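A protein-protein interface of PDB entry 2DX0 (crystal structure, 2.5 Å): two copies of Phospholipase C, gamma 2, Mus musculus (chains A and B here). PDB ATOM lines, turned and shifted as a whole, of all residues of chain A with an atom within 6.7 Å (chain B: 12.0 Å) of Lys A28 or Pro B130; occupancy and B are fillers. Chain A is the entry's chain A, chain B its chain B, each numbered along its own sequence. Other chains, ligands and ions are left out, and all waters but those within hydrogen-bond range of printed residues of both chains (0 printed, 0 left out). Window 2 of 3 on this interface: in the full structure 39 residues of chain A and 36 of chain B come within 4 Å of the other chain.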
ATOM      1  N   ASP A  12       1.872  13.792  31.050  1.00  0.00           N
ATOM      2  CA  ASP A  12       1.843  12.471  30.355  1.00  0.00           C
ATOM      3  C   ASP A  12       2.925  11.544  30.916  1.00  0.00           C
ATOM      4  O   ASP A  12       2.960  10.350  30.603  1.00  0.00           O
ATOM      5  CB  ASP A  12       2.033  12.673  28.846  1.00  0.00           C
ATOM      6  CG  ASP A  12       1.939  11.374  28.059  1.00  0.00           C
ATOM      7  OD1 ASP A  12       0.923  10.655  28.199  1.00  0.00           O
ATOM      8  OD2 ASP A  12       2.884  11.075  27.291  1.00  0.00           O
ATOM      9  N   THR A  13       3.805  12.100  31.748  1.00  0.00           N
ATOM     10  CA  THR A  13       4.866  11.320  32.378  1.00  0.00           C
ATOM     11  C   THR A  13       4.204  10.387  33.395  1.00  0.00           C
ATOM     12  O   THR A  13       3.281  10.788  34.101  1.00  0.00           O
ATOM     13  CB  THR A  13       5.870  12.226  33.117  1.00  0.00           C
ATOM     14  OG1 THR A  13       5.229  12.841  34.241  1.00  0.00           O
ATOM     15  CG2 THR A  13       6.384  13.313  32.186  1.00  0.00           C
ATOM     16  N   PHE A  25      13.887  12.753  30.380  1.00  0.00           N
ATOM     17  CA  PHE A  25      12.628  12.141  29.966  1.00  0.00           C
ATOM     18  C   PHE A  25      11.921  12.954  28.885  1.00  0.00           C
ATOM     19  O   PHE A  25      11.562  14.103  29.111  1.00  0.00           O
ATOM     20  CB  PHE A  25      11.690  11.966  31.167  1.00  0.00           C
ATOM     21  CG  PHE A  25      10.484  11.127  30.861  1.00  0.00           C
ATOM     22  CD1 PHE A  25      10.600   9.741  30.731  1.00  0.00           C
ATOM     23  CD2 PHE A  25       9.239  11.719  30.660  1.00  0.00           C
ATOM     24  CE1 PHE A  25       9.493   8.957  30.402  1.00  0.00           C
ATOM     25  CE2 PHE A  25       8.117  10.946  30.330  1.00  0.00           C
ATOM     26  CZ  PHE A  25       8.244   9.563  30.200  1.00  0.00           C
ATOM     27  N   HIS A  26      11.709  12.347  27.721  1.00  0.00           N
ATOM     28  CA  HIS A  26      11.049  13.028  26.606  1.00  0.00           C
ATOM     29  C   HIS A  26       9.879  12.258  26.015  1.00  0.00           C
ATOM     30  O   HIS A  26      10.067  11.453  25.104  1.00  0.00           O
ATOM     31  CB  HIS A  26      12.042  13.307  25.473  1.00  0.00           C
ATOM     32  CG  HIS A  26      13.236  14.098  25.896  1.00  0.00           C
ATOM     33  ND1 HIS A  26      13.139  15.371  26.414  1.00  0.00           N
ATOM     34  CD2 HIS A  26      14.554  13.793  25.889  1.00  0.00           C
ATOM     35  CE1 HIS A  26      14.347  15.815  26.710  1.00  0.00           C
ATOM     36  NE2 HIS A  26      15.225  14.877  26.401  1.00  0.00           N
ATOM     37  N   LYS A  27       8.673  12.511  26.512  1.00  0.00           N
ATOM     38  CA  LYS A  27       7.491  11.836  25.979  1.00  0.00           C
ATOM     39  C   LYS A  27       7.159  12.371  24.580  1.00  0.00           C
ATOM     40  O   LYS A  27       6.355  11.784  23.853  1.00  0.00           O
ATOM     41  CB  LYS A  27       6.298  12.023  26.924  1.00  0.00           C
ATOM     42  CG  LYS A  27       6.168  13.420  27.502  1.00  0.00           C
ATOM     43  CD  LYS A  27       5.202  13.431  28.681  1.00  0.00           C
ATOM     44  CE  LYS A  27       5.218  14.770  29.418  1.00  0.00           C
ATOM     45  NZ  LYS A  27       4.270  14.794  30.574  1.00  0.00           N
ATOM     46  N   LYS A  28       7.802  13.474  24.206  1.00  0.00           N
ATOM     47  CA  LYS A  28       7.587  14.094  22.903  1.00  0.00           C
ATOM     48  C   LYS A  28       8.268  13.306  21.776  1.00  0.00           C
ATOM     49  O   LYS A  28       7.730  13.203  20.675  1.00  0.00           O
ATOM     50  CB  LYS A  28       8.113  15.534  22.901  1.00  0.00           C
ATOM     51  CG  LYS A  28       8.237  16.186  24.281  1.00  0.00           C
ATOM     52  CD  LYS A  28       9.451  15.671  25.040  1.00  0.00           C
ATOM     53  CE  LYS A  28       9.677  16.468  26.302  1.00  0.00           C
ATOM     54  NZ  LYS A  28       8.558  16.282  27.253  1.00  0.00           N
ATOM     55  N   VAL A  29       9.453  12.762  22.047  1.00  0.00           N
ATOM     56  CA  VAL A  29      10.192  11.982  21.055  1.00  0.00           C
ATOM     57  C   VAL A  29       9.441  10.685  20.791  1.00  0.00           C
ATOM     58  O   VAL A  29       9.663   9.679  21.458  1.00  0.00           O
ATOM     59  CB  VAL A  29      11.612  11.640  21.557  1.00  0.00           C
ATOM     60  CG1 VAL A  29      12.347  10.810  20.511  1.00  0.00           C
ATOM     61  CG2 VAL A  29      12.375  12.920  21.869  1.00  0.00           C
ATOM     62  N   GLU A  30       8.565  10.701  19.795  1.00  0.00           N
ATOM     63  CA  GLU A  30       7.761   9.523  19.494  1.00  0.00           C
ATOM     64  C   GLU A  30       8.280   8.608  18.391  1.00  0.00           C
ATOM     65  O   GLU A  30       7.492   7.938  17.727  1.00  0.00           O
ATOM     66  CB  GLU A  30       6.328   9.959  19.167  1.00  0.00           C
ATOM     67  CG  GLU A  30       5.648  10.732  20.297  1.00  0.00           C
ATOM     68  CD  GLU A  30       4.211  11.117  19.974  1.00  0.00           C
ATOM     69  OE1 GLU A  30       3.989  11.798  18.946  1.00  0.00           O
ATOM     70  OE2 GLU A  30       3.305  10.741  20.752  1.00  0.00           O
ATOM     71  N   SER A  31       9.595   8.551  18.205  1.00  0.00           N
ATOM     72  CA  SER A  31      10.150   7.694  17.162  1.00  0.00           C
ATOM     73  C   SER A  31      11.602   7.308  17.405  1.00  0.00           C
ATOM     74  O   SER A  31      12.400   8.113  17.891  1.00  0.00           O
ATOM     75  CB  SER A  31      10.028   8.392  15.803  1.00  0.00           C
ATOM     76  OG  SER A  31      10.595   7.614  14.765  1.00  0.00           O
ATOM     77  N   SER A  34      13.639   9.544  15.331  1.00  0.00           N
ATOM     78  CA  SER A  34      13.663  10.880  15.911  1.00  0.00           C
ATOM     79  C   SER A  34      14.677  10.939  17.059  1.00  0.00           C
ATOM     80  O   SER A  34      15.419  11.912  17.200  1.00  0.00           O
ATOM     81  CB  SER A  34      12.266  11.239  16.417  1.00  0.00           C
ATOM     82  OG  SER A  34      12.250  12.510  17.041  1.00  0.00           O
ATOM     83  N   LEU A  38      18.055  13.446  17.387  1.00  0.00           N
ATOM     84  CA  LEU A  38      18.209  14.307  18.546  1.00  0.00           C
ATOM     85  C   LEU A  38      19.559  14.040  19.197  1.00  0.00           C
ATOM     86  O   LEU A  38      20.269  14.969  19.588  1.00  0.00           O
ATOM     87  CB  LEU A  38      17.104  14.025  19.556  1.00  0.00           C
ATOM     88  CG  LEU A  38      16.489  15.205  20.309  1.00  0.00           C
ATOM     89  CD1 LEU A  38      16.189  14.749  21.729  1.00  0.00           C
ATOM     90  CD2 LEU A  38      17.425  16.405  20.321  1.00  0.00           C
ATOM     91  N   ARG A  56      12.228   7.487  26.418  1.00  0.00           N
ATOM     92  CA  ARG A  56      11.042   7.799  25.641  1.00  0.00           C
ATOM     93  C   ARG A  56      10.096   6.614  25.716  1.00  0.00           C
ATOM     94  O   ARG A  56      10.491   5.530  26.151  1.00  0.00           O
ATOM     95  CB  ARG A  56      11.447   8.068  24.181  1.00  0.00           C
ATOM     96  CG  ARG A  56      12.301   6.950  23.577  1.00  0.00           C
ATOM     97  CD  ARG A  56      12.819   7.272  22.181  1.00  0.00           C
ATOM     98  NE  ARG A  56      12.366   6.283  21.211  1.00  0.00           N
ATOM     99  CZ  ARG A  56      13.052   5.209  20.834  1.00  0.00           C
ATOM    100  NH1 ARG A  56      14.250   4.959  21.333  1.00  0.00           N
ATOM    101  NH2 ARG A  56      12.523   4.370  19.962  1.00  0.00           N
ATOM    102  N   PRO B 126      22.135  13.825  30.429  1.00  0.00           N
ATOM    103  CA  PRO B 126      20.840  13.686  29.773  1.00  0.00           C
ATOM    104  C   PRO B 126      20.779  14.605  28.561  1.00  0.00           C
ATOM    105  O   PRO B 126      21.501  15.596  28.492  1.00  0.00           O
ATOM    106  CB  PRO B 126      19.868  14.134  30.853  1.00  0.00           C
ATOM    107  CG  PRO B 126      20.618  15.287  31.466  1.00  0.00           C
ATOM    108  CD  PRO B 126      22.038  14.722  31.595  1.00  0.00           C
ATOM    109  N   VAL B 127      19.934  14.258  27.598  1.00  0.00           N
ATOM    110  CA  VAL B 127      19.745  15.104  26.434  1.00  0.00           C
ATOM    111  C   VAL B 127      18.630  16.033  26.921  1.00  0.00           C
ATOM    112  O   VAL B 127      17.568  15.572  27.338  1.00  0.00           O
ATOM    113  CB  VAL B 127      19.284  14.295  25.211  1.00  0.00           C
ATOM    114  CG1 VAL B 127      19.163  15.201  24.007  1.00  0.00           C
ATOM    115  CG2 VAL B 127      20.270  13.193  24.929  1.00  0.00           C
ATOM    116  N   PRO B 128      18.871  17.354  26.883  1.00  0.00           N
ATOM    117  CA  PRO B 128      18.001  18.464  27.298  1.00  0.00           C
ATOM    118  C   PRO B 128      16.533  18.519  26.858  1.00  0.00           C
ATOM    119  O   PRO B 128      15.638  18.260  27.664  1.00  0.00           O
ATOM    120  CB  PRO B 128      18.783  19.697  26.842  1.00  0.00           C
ATOM    121  CG  PRO B 128      19.493  19.205  25.633  1.00  0.00           C
ATOM    122  CD  PRO B 128      20.016  17.877  26.117  1.00  0.00           C
ATOM    123  N   ASN B 129      16.275  18.882  25.602  1.00  0.00           N
ATOM    124  CA  ASN B 129      14.891  18.991  25.131  1.00  0.00           C
ATOM    125  C   ASN B 129      14.629  18.187  23.862  1.00  0.00           C
ATOM    126  O   ASN B 129      15.547  17.916  23.089  1.00  0.00           O
ATOM    127  CB  ASN B 129      14.527  20.464  24.885  1.00  0.00           C
ATOM    128  CG  ASN B 129      14.974  20.959  23.520  1.00  0.00           C
ATOM    129  OD1 ASN B 129      16.127  20.770  23.124  1.00  0.00           O
ATOM    130  ND2 ASN B 129      14.062  21.603  22.795  1.00  0.00           N
ATOM    131  N   PRO B 130      13.360  17.805  23.629  1.00  0.00           N
ATOM    132  CA  PRO B 130      12.970  17.025  22.450  1.00  0.00           C
ATOM    133  C   PRO B 130      13.184  17.785  21.146  1.00  0.00           C
ATOM    134  O   PRO B 130      13.684  18.930  21.207  1.00  0.00           O
ATOM    135  CB  PRO B 130      11.496  16.727  22.712  1.00  0.00           C
ATOM    136  CG  PRO B 130      11.046  17.961  23.417  1.00  0.00           C
ATOM    137  CD  PRO B 130      12.170  18.197  24.406  1.00  0.00           C
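Of the printed residues of chain B, Lys A28 touches Pro B130.
Of the printed residues of chain A, Pro B130 touches His A26 (3.6 Å), Lys A28 (3.2 Å) and Val A29 (3.997 Å).
No residue of chain B comes within 4 Å of Phe A25.
Of chain B, only Val B127 (2.6 Å), Pro B128 (2.9 Å), Asn B129 (3.6 Å) and Pro B130 (3.6 Å) come within 4 Å of His A26.
No residue of chain B comes within 4 Å of Lys A27.
No residue of chain B comes within 4 Å of Glu A30.
Printed residues of chain B within 4 Å of Val A29: Pro B130 (3.997 Å).
Printed residues of chain A within 4 Å of Pro B128: His A26.
No position is printed for both chains.
Among the printed residues, pairs that only touch across the chains: His A26 with Pro B128 (2.9 Å), His A26 with Asn B129 (3.6 Å), His A26 with Pro B130 (3.6 Å), Lys A28 with Pro B130 (3.2 Å), Val A29 with Pro B130 (3.997 Å), Leu A38 with Val B127 (3.8 Å) and Leu A38 with Asn B129 (3.5 Å).
The backbone carbonyl oxygen (O) of Val B127 lies within hydrogen-bond range of a ring nitrogen (NE2) of His A26 (2.6 Å).
Hydrophobic or aromatic side chains of chain B within 4 Å of the printed part of chain A: Val B127 and Pro B130.
Along chain B the printed residues that touch a printed residue of chain A span positions 127 to 130.
Among the printed residues, no Asp or Glu carboxylate lies within 4 Å of a Lys or Arg side-chain nitrogen of the other chain.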
